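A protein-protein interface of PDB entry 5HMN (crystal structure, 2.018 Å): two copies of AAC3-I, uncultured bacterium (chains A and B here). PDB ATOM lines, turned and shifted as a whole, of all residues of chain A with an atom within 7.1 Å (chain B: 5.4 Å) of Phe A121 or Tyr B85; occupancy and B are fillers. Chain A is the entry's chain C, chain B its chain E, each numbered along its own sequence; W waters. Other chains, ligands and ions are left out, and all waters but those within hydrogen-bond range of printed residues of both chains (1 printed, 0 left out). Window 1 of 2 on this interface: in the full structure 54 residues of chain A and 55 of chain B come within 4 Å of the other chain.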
ATOM      1  N   ALA A  71       0.401  14.281  -9.176  1.00  0.00           N
ATOM      2  CA  ALA A  71       0.142  15.333  -8.200  1.00  0.00           C
ATOM      3  C   ALA A  71       0.389  16.726  -8.775  1.00  0.00           C
ATOM      4  O   ALA A  71       1.121  16.886  -9.752  1.00  0.00           O
ATOM      5  CB  ALA A  71       0.995  15.122  -6.959  1.00  0.00           C
ATOM      6  N   TYR A  72      -0.221  17.724  -8.149  1.00  0.00           N
ATOM      7  CA  TYR A  72      -0.081  19.114  -8.575  1.00  0.00           C
ATOM      8  C   TYR A  72       0.412  19.964  -7.415  1.00  0.00           C
ATOM      9  O   TYR A  72      -0.154  19.920  -6.323  1.00  0.00           O
ATOM     10  CB  TYR A  72      -1.414  19.660  -9.095  1.00  0.00           C
ATOM     11  CG  TYR A  72      -1.947  18.968 -10.336  1.00  0.00           C
ATOM     12  CD1 TYR A  72      -2.726  17.825 -10.238  1.00  0.00           C
ATOM     13  CD2 TYR A  72      -1.686  19.475 -11.605  1.00  0.00           C
ATOM     14  CE1 TYR A  72      -3.217  17.191 -11.372  1.00  0.00           C
ATOM     15  CE2 TYR A  72      -2.174  18.853 -12.740  1.00  0.00           C
ATOM     16  CZ  TYR A  72      -2.937  17.711 -12.617  1.00  0.00           C
ATOM     17  OH  TYR A  72      -3.426  17.089 -13.745  1.00  0.00           O
ATOM     18  N   LEU A  74       0.509  23.363  -5.625  1.00  0.00           N
ATOM     19  CA  LEU A  74      -0.302  24.575  -5.602  1.00  0.00           C
ATOM     20  C   LEU A  74       0.408  25.688  -4.845  1.00  0.00           C
ATOM     21  O   LEU A  74       0.418  25.704  -3.613  1.00  0.00           O
ATOM     22  CB  LEU A  74      -1.667  24.289  -4.966  1.00  0.00           C
ATOM     23  CG  LEU A  74      -2.829  23.846  -5.863  1.00  0.00           C
ATOM     24  CD1 LEU A  74      -2.437  22.736  -6.811  1.00  0.00           C
ATOM     25  CD2 LEU A  74      -4.021  23.425  -5.013  1.00  0.00           C
ATOM     26  N   LYS A  76       0.589  29.028  -3.177  1.00  0.00           N
ATOM     27  CA  LYS A  76      -0.512  29.758  -2.555  1.00  0.00           C
ATOM     28  C   LYS A  76      -0.408  31.276  -2.723  1.00  0.00           C
ATOM     29  O   LYS A  76       0.656  31.812  -3.030  1.00  0.00           O
ATOM     30  CB  LYS A  76      -0.603  29.403  -1.069  1.00  0.00           C
ATOM     31  CG  LYS A  76      -0.751  27.907  -0.787  1.00  0.00           C
ATOM     32  CD  LYS A  76      -2.000  27.305  -1.440  1.00  0.00           C
ATOM     33  CE  LYS A  76      -3.283  27.990  -0.972  1.00  0.00           C
ATOM     34  NZ  LYS A  76      -3.534  27.858   0.493  1.00  0.00           N
ATOM     35  N   GLU A  83       1.372  23.832  -1.421  1.00  0.00           N
ATOM     36  CA  GLU A  83       0.888  22.514  -1.039  1.00  0.00           C
ATOM     37  C   GLU A  83       0.830  21.607  -2.256  1.00  0.00           C
ATOM     38  O   GLU A  83       0.616  22.076  -3.377  1.00  0.00           O
ATOM     39  CB  GLU A  83      -0.499  22.597  -0.406  1.00  0.00           C
ATOM     40  CG  GLU A  83      -0.799  23.899   0.295  1.00  0.00           C
ATOM     41  CD  GLU A  83      -2.268  24.024   0.646  1.00  0.00           C
ATOM     42  OE1 GLU A  83      -3.087  23.289   0.054  1.00  0.00           O
ATOM     43  OE2 GLU A  83      -2.604  24.858   1.512  1.00  0.00           O
ATOM     44  N   ILE A  84       1.005  20.312  -2.030  1.00  0.00           N
ATOM     45  CA  ILE A  84       0.956  19.343  -3.118  1.00  0.00           C
ATOM     46  C   ILE A  84      -0.347  18.555  -3.046  1.00  0.00           C
ATOM     47  O   ILE A  84      -0.669  17.941  -2.027  1.00  0.00           O
ATOM     48  CB  ILE A  84       2.158  18.384  -3.084  1.00  0.00           C
ATOM     49  CG1 ILE A  84       3.466  19.167  -3.196  1.00  0.00           C
ATOM     50  CG2 ILE A  84       2.060  17.357  -4.206  1.00  0.00           C
ATOM     51  CD1 ILE A  84       4.696  18.293  -3.153  1.00  0.00           C
ATOM     52  N   TYR A  85      -1.108  18.605  -4.130  1.00  0.00           N
ATOM     53  CA  TYR A  85      -2.365  17.880  -4.215  1.00  0.00           C
ATOM     54  C   TYR A  85      -2.187  16.567  -4.975  1.00  0.00           C
ATOM     55  O   TYR A  85      -1.930  16.565  -6.176  1.00  0.00           O
ATOM     56  CB  TYR A  85      -3.425  18.755  -4.888  1.00  0.00           C
ATOM     57  CG  TYR A  85      -4.756  18.077  -5.118  1.00  0.00           C
ATOM     58  CD1 TYR A  85      -5.369  17.341  -4.114  1.00  0.00           C
ATOM     59  CD2 TYR A  85      -5.414  18.200  -6.331  1.00  0.00           C
ATOM     60  CE1 TYR A  85      -6.591  16.731  -4.320  1.00  0.00           C
ATOM     61  CE2 TYR A  85      -6.635  17.594  -6.547  1.00  0.00           C
ATOM     62  CZ  TYR A  85      -7.221  16.860  -5.537  1.00  0.00           C
ATOM     63  OH  TYR A  85      -8.442  16.254  -5.744  1.00  0.00           O
ATOM     64  N   ILE A  86      -2.318  15.452  -4.268  1.00  0.00           N
ATOM     65  CA  ILE A  86      -2.352  14.149  -4.919  1.00  0.00           C
ATOM     66  C   ILE A  86      -3.674  13.978  -5.658  1.00  0.00           C
ATOM     67  O   ILE A  86      -4.742  13.925  -5.041  1.00  0.00           O
ATOM     68  CB  ILE A  86      -2.176  13.001  -3.910  1.00  0.00           C
ATOM     69  CG1 ILE A  86      -0.826  13.123  -3.199  1.00  0.00           C
ATOM     70  CG2 ILE A  86      -2.290  11.660  -4.611  1.00  0.00           C
ATOM     71  CD1 ILE A  86      -0.539  11.993  -2.215  1.00  0.00           C
ATOM     72  N   TYR A  87      -3.610  13.909  -6.983  1.00  0.00           N
ATOM     73  CA  TYR A  87      -4.820  13.717  -7.761  1.00  0.00           C
ATOM     74  C   TYR A  87      -5.164  12.238  -7.880  1.00  0.00           C
ATOM     75  O   TYR A  87      -6.251  11.829  -7.489  1.00  0.00           O
ATOM     76  CB  TYR A  87      -4.694  14.336  -9.153  1.00  0.00           C
ATOM     77  CG  TYR A  87      -6.034  14.451  -9.851  1.00  0.00           C
ATOM     78  CD1 TYR A  87      -6.792  15.614  -9.756  1.00  0.00           C
ATOM     79  CD2 TYR A  87      -6.559  13.385 -10.574  1.00  0.00           C
ATOM     80  CE1 TYR A  87      -8.028  15.713 -10.381  1.00  0.00           C
ATOM     81  CE2 TYR A  87      -7.785  13.475 -11.199  1.00  0.00           C
ATOM     82  CZ  TYR A  87      -8.518  14.637 -11.102  1.00  0.00           C
ATOM     83  OH  TYR A  87      -9.746  14.718 -11.725  1.00  0.00           O
ATOM     84  N   LEU A 108       7.178  11.489  -2.579  1.00  0.00           N
ATOM     85  CA  LEU A 108       6.528  12.776  -2.805  1.00  0.00           C
ATOM     86  C   LEU A 108       6.855  13.748  -1.672  1.00  0.00           C
ATOM     87  O   LEU A 108       6.958  14.954  -1.890  1.00  0.00           O
ATOM     88  CB  LEU A 108       5.015  12.596  -2.936  1.00  0.00           C
ATOM     89  CG  LEU A 108       4.233  13.825  -3.405  1.00  0.00           C
ATOM     90  CD1 LEU A 108       4.711  14.261  -4.782  1.00  0.00           C
ATOM     91  CD2 LEU A 108       2.742  13.543  -3.418  1.00  0.00           C
ATOM     92  N   VAL A 119       2.880  20.941   3.118  1.00  0.00           N
ATOM     93  CA  VAL A 119       1.880  19.899   3.327  1.00  0.00           C
ATOM     94  C   VAL A 119       1.478  19.212   2.020  1.00  0.00           C
ATOM     95  O   VAL A 119       1.540  19.794   0.935  1.00  0.00           O
ATOM     96  CB  VAL A 119       0.614  20.473   4.030  1.00  0.00           C
ATOM     97  CG1 VAL A 119      -0.182  21.347   3.081  1.00  0.00           C
ATOM     98  CG2 VAL A 119      -0.257  19.359   4.604  1.00  0.00           C
ATOM     99  N   ILE A 120       1.100  17.947   2.136  1.00  0.00           N
ATOM    100  CA  ILE A 120       0.530  17.206   1.026  1.00  0.00           C
ATOM    101  C   ILE A 120      -0.896  16.826   1.394  1.00  0.00           C
ATOM    102  O   ILE A 120      -1.144  16.349   2.500  1.00  0.00           O
ATOM    103  CB  ILE A 120       1.355  15.944   0.707  1.00  0.00           C
ATOM    104  CG1 ILE A 120       2.774  16.331   0.284  1.00  0.00           C
ATOM    105  CG2 ILE A 120       0.672  15.115  -0.374  1.00  0.00           C
ATOM    106  CD1 ILE A 120       3.707  15.136   0.111  1.00  0.00           C
ATOM    107  N   PHE A 121      -1.844  17.051   0.491  1.00  0.00           N
ATOM    108  CA  PHE A 121      -3.214  16.649   0.782  1.00  0.00           C
ATOM    109  C   PHE A 121      -3.824  15.849  -0.366  1.00  0.00           C
ATOM    110  O   PHE A 121      -3.384  15.927  -1.518  1.00  0.00           O
ATOM    111  CB  PHE A 121      -4.081  17.866   1.135  1.00  0.00           C
ATOM    112  CG  PHE A 121      -4.358  18.789  -0.020  1.00  0.00           C
ATOM    113  CD1 PHE A 121      -5.572  18.740  -0.683  1.00  0.00           C
ATOM    114  CD2 PHE A 121      -3.413  19.713  -0.431  1.00  0.00           C
ATOM    115  CE1 PHE A 121      -5.840  19.592  -1.742  1.00  0.00           C
ATOM    116  CE2 PHE A 121      -3.670  20.565  -1.493  1.00  0.00           C
ATOM    117  CZ  PHE A 121      -4.888  20.504  -2.148  1.00  0.00           C
ATOM    118  N   VAL A 122      -4.819  15.043  -0.026  1.00  0.00           N
ATOM    119  CA  VAL A 122      -5.444  14.156  -0.992  1.00  0.00           C
ATOM    120  C   VAL A 122      -6.875  13.854  -0.559  1.00  0.00           C
ATOM    121  O   VAL A 122      -7.146  13.643   0.625  1.00  0.00           O
ATOM    122  CB  VAL A 122      -4.643  12.837  -1.159  1.00  0.00           C
ATOM    123  CG1 VAL A 122      -4.440  12.151   0.186  1.00  0.00           C
ATOM    124  CG2 VAL A 122      -5.328  11.899  -2.142  1.00  0.00           C
ATOM    125  N   GLN A 123      -7.794  13.874  -1.516  1.00  0.00           N
ATOM    126  CA  GLN A 123      -9.179  13.522  -1.246  1.00  0.00           C
ATOM    127  C   GLN A 123      -9.364  12.021  -1.380  1.00  0.00           C
ATOM    128  O   GLN A 123      -8.919  11.412  -2.349  1.00  0.00           O
ATOM    129  CB  GLN A 123     -10.131  14.250  -2.195  1.00  0.00           C
ATOM    130  CG  GLN A 123     -10.111  15.759  -2.089  1.00  0.00           C
ATOM    131  CD  GLN A 123     -11.222  16.403  -2.898  1.00  0.00           C
ATOM    132  OE1 GLN A 123     -12.282  15.807  -3.098  1.00  0.00           O
ATOM    133  NE2 GLN A 123     -10.982  17.620  -3.376  1.00  0.00           N
ATOM    134  N   HIS A 148     -17.808  17.615  -1.475  1.00  0.00           N
ATOM    135  CA  HIS A 148     -17.267  17.839  -2.796  1.00  0.00           C
ATOM    136  C   HIS A 148     -18.371  18.057  -3.823  1.00  0.00           C
ATOM    137  O   HIS A 148     -19.320  17.344  -3.837  1.00  0.00           O
ATOM    138  CB  HIS A 148     -16.409  16.658  -3.185  1.00  0.00           C
ATOM    139  CG  HIS A 148     -15.773  16.791  -4.522  1.00  0.00           C
ATOM    140  ND1 HIS A 148     -14.550  17.387  -4.701  1.00  0.00           N
ATOM    141  CD2 HIS A 148     -16.179  16.392  -5.742  1.00  0.00           C
ATOM    142  CE1 HIS A 148     -14.234  17.362  -5.978  1.00  0.00           C
ATOM    143  NE2 HIS A 148     -15.208  16.765  -6.632  1.00  0.00           N
ATOM    144  N   ALA B  70     -10.496  32.358  -5.870  1.00  0.00           N
ATOM    145  CA  ALA B  70      -9.157  31.928  -6.238  1.00  0.00           C
ATOM    146  C   ALA B  70      -9.200  30.467  -6.653  1.00  0.00           C
ATOM    147  O   ALA B  70      -9.668  29.615  -5.892  1.00  0.00           O
ATOM    148  CB  ALA B  70      -8.185  32.136  -5.092  1.00  0.00           C
ATOM    149  N   ALA B  71      -8.721  30.183  -7.861  1.00  0.00           N
ATOM    150  CA  ALA B  71      -8.812  28.842  -8.421  1.00  0.00           C
ATOM    151  C   ALA B  71      -7.521  28.407  -9.110  1.00  0.00           C
ATOM    152  O   ALA B  71      -6.654  29.227  -9.411  1.00  0.00           O
ATOM    153  CB  ALA B  71      -9.976  28.766  -9.403  1.00  0.00           C
ATOM    154  N   TYR B  72      -7.412  27.106  -9.359  1.00  0.00           N
ATOM    155  CA  TYR B  72      -6.276  26.543 -10.083  1.00  0.00           C
ATOM    156  C   TYR B  72      -6.756  25.672 -11.236  1.00  0.00           C
ATOM    157  O   TYR B  72      -7.586  24.782 -11.047  1.00  0.00           O
ATOM    158  CB  TYR B  72      -5.388  25.715  -9.154  1.00  0.00           C
ATOM    159  CG  TYR B  72      -4.769  26.497  -8.024  1.00  0.00           C
ATOM    160  CD1 TYR B  72      -5.436  26.654  -6.815  1.00  0.00           C
ATOM    161  CD2 TYR B  72      -3.511  27.067  -8.158  1.00  0.00           C
ATOM    162  CE1 TYR B  72      -4.873  27.361  -5.773  1.00  0.00           C
ATOM    163  CE2 TYR B  72      -2.937  27.779  -7.118  1.00  0.00           C
ATOM    164  CZ  TYR B  72      -3.625  27.924  -5.931  1.00  0.00           C
ATOM    165  OH  TYR B  72      -3.065  28.629  -4.889  1.00  0.00           O
ATOM    166  N   GLU B  73      -6.233  25.930 -12.426  1.00  0.00           N
ATOM    167  CA  GLU B  73      -6.521  25.079 -13.569  1.00  0.00           C
ATOM    168  C   GLU B  73      -5.634  23.847 -13.515  1.00  0.00           C
ATOM    169  O   GLU B  73      -4.412  23.956 -13.543  1.00  0.00           O
ATOM    170  CB  GLU B  73      -6.303  25.820 -14.887  1.00  0.00           C
ATOM    171  CG  GLU B  73      -6.632  24.974 -16.108  1.00  0.00           C
ATOM    172  CD  GLU B  73      -6.183  25.609 -17.411  1.00  0.00           C
ATOM    173  OE1 GLU B  73      -5.601  26.715 -17.372  1.00  0.00           O
ATOM    174  OE2 GLU B  73      -6.409  24.996 -18.475  1.00  0.00           O
ATOM    175  N   LEU B  74      -6.255  22.681 -13.420  1.00  0.00           N
ATOM    176  CA  LEU B  74      -5.511  21.426 -13.383  1.00  0.00           C
ATOM    177  C   LEU B  74      -5.570  20.751 -14.748  1.00  0.00           C
ATOM    178  O   LEU B  74      -6.581  20.157 -15.113  1.00  0.00           O
ATOM    179  CB  LEU B  74      -6.067  20.505 -12.295  1.00  0.00           C
ATOM    180  CG  LEU B  74      -5.470  20.610 -10.886  1.00  0.00           C
ATOM    181  CD1 LEU B  74      -5.272  22.045 -10.441  1.00  0.00           C
ATOM    182  CD2 LEU B  74      -6.345  19.864  -9.887  1.00  0.00           C
ATOM    183  N   GLU B  83      -9.355  20.690 -15.453  1.00  0.00           N
ATOM    184  CA  GLU B  83     -10.300  20.769 -14.348  1.00  0.00           C
ATOM    185  C   GLU B  83      -9.981  21.974 -13.478  1.00  0.00           C
ATOM    186  O   GLU B  83      -8.839  22.157 -13.053  1.00  0.00           O
ATOM    187  CB  GLU B  83     -10.270  19.487 -13.515  1.00  0.00           C
ATOM    188  CG  GLU B  83     -10.591  18.233 -14.312  1.00  0.00           C
ATOM    189  CD  GLU B  83     -10.592  16.979 -13.459  1.00  0.00           C
ATOM    190  OE1 GLU B  83     -10.488  17.101 -12.223  1.00  0.00           O
ATOM    191  OE2 GLU B  83     -10.691  15.868 -14.027  1.00  0.00           O
ATOM    192  N   ILE B  84     -10.990  22.800 -13.217  1.00  0.00           N
ATOM    193  CA  ILE B  84     -10.798  23.990 -12.405  1.00  0.00           C
ATOM    194  C   ILE B  84     -11.064  23.709 -10.930  1.00  0.00           C
ATOM    195  O   ILE B  84     -12.184  23.375 -10.540  1.00  0.00           O
ATOM    196  CB  ILE B  84     -11.716  25.136 -12.864  1.00  0.00           C
ATOM    197  CG1 ILE B  84     -11.608  25.332 -14.379  1.00  0.00           C
ATOM    198  CG2 ILE B  84     -11.381  26.409 -12.109  1.00  0.00           C
ATOM    199  CD1 ILE B  84     -10.221  25.706 -14.855  1.00  0.00           C
ATOM    200  N   TYR B  85     -10.027  23.850 -10.113  1.00  0.00           N
ATOM    201  CA  TYR B  85     -10.151  23.658  -8.675  1.00  0.00           C
ATOM    202  C   TYR B  85     -10.315  25.003  -7.963  1.00  0.00           C
ATOM    203  O   TYR B  85      -9.359  25.764  -7.839  1.00  0.00           O
ATOM    204  CB  TYR B  85      -8.927  22.914  -8.129  1.00  0.00           C
ATOM    205  CG  TYR B  85      -8.973  22.606  -6.643  1.00  0.00           C
ATOM    206  CD1 TYR B  85     -10.178  22.552  -5.954  1.00  0.00           C
ATOM    207  CD2 TYR B  85      -7.805  22.375  -5.930  1.00  0.00           C
ATOM    208  CE1 TYR B  85     -10.218  22.274  -4.601  1.00  0.00           C
ATOM    209  CE2 TYR B  85      -7.835  22.096  -4.576  1.00  0.00           C
ATOM    210  CZ  TYR B  85      -9.046  22.048  -3.916  1.00  0.00           C
ATOM    211  OH  TYR B  85      -9.084  21.771  -2.568  1.00  0.00           O
ATOM    212  N   ILE B  86     -11.529  25.291  -7.502  1.00  0.00           N
ATOM    213  CA  ILE B  86     -11.758  26.476  -6.679  1.00  0.00           C
ATOM    214  C   ILE B  86     -11.191  26.239  -5.287  1.00  0.00           C
ATOM    215  O   ILE B  86     -11.651  25.351  -4.567  1.00  0.00           O
ATOM    216  CB  ILE B  86     -13.254  26.825  -6.555  1.00  0.00           C
ATOM    217  CG1 ILE B  86     -13.854  27.113  -7.932  1.00  0.00           C
ATOM    218  CG2 ILE B  86     -13.438  28.023  -5.637  1.00  0.00           C
ATOM    219  CD1 ILE B  86     -15.306  27.496  -7.900  1.00  0.00           C
ATOM    220  N   TYR B  87     -10.185  27.016  -4.907  1.00  0.00           N
ATOM    221  CA  TYR B  87      -9.592  26.845  -3.587  1.00  0.00           C
ATOM    222  C   TYR B  87     -10.347  27.654  -2.543  1.00  0.00           C
ATOM    223  O   TYR B  87     -10.700  27.137  -1.486  1.00  0.00           O
ATOM    224  CB  TYR B  87      -8.114  27.237  -3.585  1.00  0.00           C
ATOM    225  CG  TYR B  87      -7.373  26.661  -2.402  1.00  0.00           C
ATOM    226  CD1 TYR B  87      -6.686  25.460  -2.507  1.00  0.00           C
ATOM    227  CD2 TYR B  87      -7.389  27.300  -1.170  1.00  0.00           C
ATOM    228  CE1 TYR B  87      -6.017  24.922  -1.425  1.00  0.00           C
ATOM    229  CE2 TYR B  87      -6.727  26.772  -0.084  1.00  0.00           C
ATOM    230  CZ  TYR B  87      -6.041  25.584  -0.217  1.00  0.00           C
ATOM    231  OH  TYR B  87      -5.380  25.057   0.866  1.00  0.00           O
ATOM    232  N   PHE B 121     -14.677  21.988  -9.793  1.00  0.00           N
ATOM    233  CA  PHE B 121     -15.004  21.387  -8.508  1.00  0.00           C
ATOM    234  C   PHE B 121     -14.497  22.238  -7.353  1.00  0.00           C
ATOM    235  O   PHE B 121     -13.498  22.947  -7.463  1.00  0.00           O
ATOM    236  CB  PHE B 121     -14.471  19.949  -8.415  1.00  0.00           C
ATOM    237  CG  PHE B 121     -12.981  19.828  -8.533  1.00  0.00           C
ATOM    238  CD1 PHE B 121     -12.186  19.787  -7.399  1.00  0.00           C
ATOM    239  CD2 PHE B 121     -12.376  19.718  -9.775  1.00  0.00           C
ATOM    240  CE1 PHE B 121     -10.809  19.657  -7.503  1.00  0.00           C
ATOM    241  CE2 PHE B 121     -11.003  19.593  -9.885  1.00  0.00           C
ATOM    242  CZ  PHE B 121     -10.218  19.564  -8.747  1.00  0.00           C
ATOM    243  N   VAL B 122     -15.226  22.192  -6.248  1.00  0.00           N
ATOM    244  CA  VAL B 122     -14.892  22.991  -5.084  1.00  0.00           C
ATOM    245  C   VAL B 122     -15.201  22.199  -3.822  1.00  0.00           C
ATOM    246  O   VAL B 122     -16.203  21.486  -3.756  1.00  0.00           O
ATOM    247  CB  VAL B 122     -15.660  24.335  -5.082  1.00  0.00           C
ATOM    248  CG1 VAL B 122     -17.161  24.102  -5.168  1.00  0.00           C
ATOM    249  CG2 VAL B 122     -15.309  25.162  -3.849  1.00  0.00           C
ATOM    250  N   GLN B 123     -14.394  22.328  -2.787  1.00  0.00           N
ATOM    251  CA  GLN B 123     -14.644  21.648  -1.534  1.00  0.00           C
ATOM    252  C   GLN B 123     -15.353  22.556  -0.579  1.00  0.00           C
ATOM    253  O   GLN B 123     -15.174  23.721  -0.514  1.00  0.00           O
ATOM    254  CB  GLN B 123     -13.385  21.170  -0.820  1.00  0.00           C
ATOM    255  CG  GLN B 123     -12.667  19.962  -1.390  1.00  0.00           C
ATOM    256  CD  GLN B 123     -11.604  19.415  -0.432  1.00  0.00           C
ATOM    257  OE1 GLN B 123     -11.200  18.253  -0.503  1.00  0.00           O
ATOM    258  NE2 GLN B 123     -11.138  20.259   0.448  1.00  0.00           N
ATOM    259  N   HIS B 148     -11.020  14.034   3.374  1.00  0.00           N
ATOM    260  CA  HIS B 148      -9.884  14.864   3.107  1.00  0.00           C
ATOM    261  C   HIS B 148      -8.759  14.538   4.062  1.00  0.00           C
ATOM    262  O   HIS B 148      -8.978  14.425   5.226  1.00  0.00           O
ATOM    263  CB  HIS B 148     -10.276  16.310   3.256  1.00  0.00           C
ATOM    264  CG  HIS B 148      -9.221  17.272   2.839  1.00  0.00           C
ATOM    265  ND1 HIS B 148      -8.399  17.898   3.733  1.00  0.00           N
ATOM    266  CD2 HIS B 148      -8.878  17.744   1.625  1.00  0.00           C
ATOM    267  CE1 HIS B 148      -7.582  18.702   3.093  1.00  0.00           C
ATOM    268  NE2 HIS B 148      -7.851  18.626   1.813  1.00  0.00           N
ATOM    269  N   PHE B 149      -7.552  14.367   3.561  1.00  0.00           N
ATOM    270  CA  PHE B 149      -6.400  14.023   4.390  1.00  0.00           C
ATOM    271  C   PHE B 149      -5.253  15.016   4.224  1.00  0.00           C
ATOM    272  O   PHE B 149      -4.843  15.323   3.105  1.00  0.00           O
ATOM    273  CB  PHE B 149      -5.907  12.613   4.062  1.00  0.00           C
ATOM    274  CG  PHE B 149      -6.851  11.524   4.479  1.00  0.00           C
ATOM    275  CD1 PHE B 149      -6.722  10.918   5.714  1.00  0.00           C
ATOM    276  CD2 PHE B 149      -7.866  11.100   3.632  1.00  0.00           C
ATOM    277  CE1 PHE B 149      -7.584   9.911   6.101  1.00  0.00           C
ATOM    278  CE2 PHE B 149      -8.733  10.095   4.018  1.00  0.00           C
ATOM    279  CZ  PHE B 149      -8.588   9.501   5.252  1.00  0.00           C
ATOM    280  N   ASP B 150      -4.738  15.517   5.342  1.00  0.00           N
ATOM    281  CA  ASP B 150      -3.581  16.403   5.310  1.00  0.00           C
ATOM    282  C   ASP B 150      -2.338  15.665   5.785  1.00  0.00           C
ATOM    283  O   ASP B 150      -2.208  15.346   6.965  1.00  0.00           O
ATOM    284  CB  ASP B 150      -3.823  17.647   6.168  1.00  0.00           C
ATOM    285  CG  ASP B 150      -4.951  18.514   5.633  1.00  0.00           C
ATOM    286  OD1 ASP B 150      -4.821  19.019   4.497  1.00  0.00           O
ATOM    287  OD2 ASP B 150      -5.962  18.694   6.347  1.00  0.00           O
ATOM    288  N   ILE B 151      -1.429  15.396   4.857  1.00  0.00           N
ATOM    289  CA  ILE B 151      -0.200  14.675   5.165  1.00  0.00           C
ATOM    290  C   ILE B 151       0.993  15.626   5.280  1.00  0.00           C
ATOM    291  O   ILE B 151       1.351  16.312   4.320  1.00  0.00           O
ATOM    292  CB  ILE B 151       0.099  13.605   4.098  1.00  0.00           C
ATOM    293  CG1 ILE B 151      -1.135  12.723   3.866  1.00  0.00           C
ATOM    294  CG2 ILE B 151       1.290  12.768   4.512  1.00  0.00           C
ATOM    295  CD1 ILE B 151      -0.969  11.711   2.745  1.00  0.00           C
HETATM  296  O   HOH W   1      -4.594  26.509   3.354  1.00  0.00           O
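The side-chain carboxylate (OE2) of Glu A83 sits at hydrogen-bond distance from the side-chain hydroxyl (OH) of Tyr B87, 2.9 Å away. The side-chain amide nitrogen (NE2) of Gln A123 is in hydrogen-bond range of the side-chain amide oxygen (OE1) of Gln B123, at 2.9 Å. The backbone carbonyl oxygen (O) of Ile A120 lies within hydrogen-bond range of the backbone NH (N) of Ile B151 (2.6 Å). O of Val A122 is in hydrogen-bond range of N of Phe B149 (3.1 Å). The side-chain amino group of Lys A76 sits at hydrogen-bond distance from the side-chain hydroxyl of Tyr B87 (3.4 Å). OH of Tyr A87 is in hydrogen-bond range of OE1 of Glu B83, at 2.5 Å.
The backbone NH (N) of Phe A121 lies within hydrogen-bond range of the backbone carbonyl oxygen (O) of Ile A84 (2.9 Å). N of Tyr B85 lies within hydrogen-bond range of O of Tyr B72. A ring nitrogen (ND1) of His A148 sits at hydrogen-bond distance from the side-chain amide oxygen of Gln A123. O of Tyr A72 lies within hydrogen-bond range of N of Tyr A85 (2.7 Å). The side-chain amino group (NZ) of Lys A76 lies within salt-bridge range of the side-chain carboxylate (OE2) of Glu A83 (3.3 Å). The backbone carbonyl oxygen (O) of Ile B84 sits at hydrogen-bond distance from the backbone NH (N) of Phe B121 (2.9 Å).
Among the printed residues, pairs that only touch across the chains: Tyr A72 with Leu B74 (3.9 Å), Leu A74 with Tyr B72 (3.9 Å), Lys A76 with Tyr B72 (3.6 Å), Val A119 with Ile B151 (3.5 Å), Ile A120 with Phe B149 (3.9 Å), Ile A120 with Asp B150 (3.6 Å), Phe A121 with Tyr B85 (3.99 Å), Phe A121 with His B148 (3.4 Å), Phe A121 with Phe B149 (3.1 Å), Phe A121 with Asp B150 (3.6 Å), Val A122 with His B148 (3.9 Å), His A148 with Phe B121 (3.5 Å) and His A148 with Val B122 (3.9 Å).
Of the printed residues of chain B, Val A119 touches Ile B151. Of the printed residues of chain A, Tyr B85 touches Phe A121. Printed residues of chain A within 4 Å of His B148: Phe A121 and Val A122. The nearest printed residue of chain A that does not touch Tyr B85 is Leu A74 (4.03 Å). The nearest printed residue of chain B that does not touch Val A119 is Asp B150 (4.3 Å).
Printed residues of chain B that touch a printed residue of chain A: Tyr B72, Leu B74, Glu B83, Tyr B85, Tyr B87, Phe B121, Val B122, Gln B123, His B148, Phe B149, Asp B150 and Ile B151. Printed residues of chain A that touch a printed residue of chain B: Tyr A72, Leu A74, Lys A76, Glu A83, Tyr A87, Val A119, Ile A120, Phe A121, Val A122, Gln A123 and His A148. Among the printed residues, no Asp or Glu carboxylate lies within 4 Å of a Lys or Arg side-chain nitrogen of the other chain.
Tyr A72 touches Leu B74, and with the chains exchanged Leu A74 touches Tyr B72. Glu A83 touches Tyr B87, and with the chains exchanged Tyr A87 touches Glu B83. Val A122 touches His B148, and with the chains exchanged His A148 touches Val B122. Gln A123 touches its own counterpart, Gln B123.
Water W1 lies within hydrogen-bond range of OH of Tyr B87 (3.0 Å), OE2 of Glu A83 (3.2 Å) and NZ of Lys A76 (3.3 Å).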
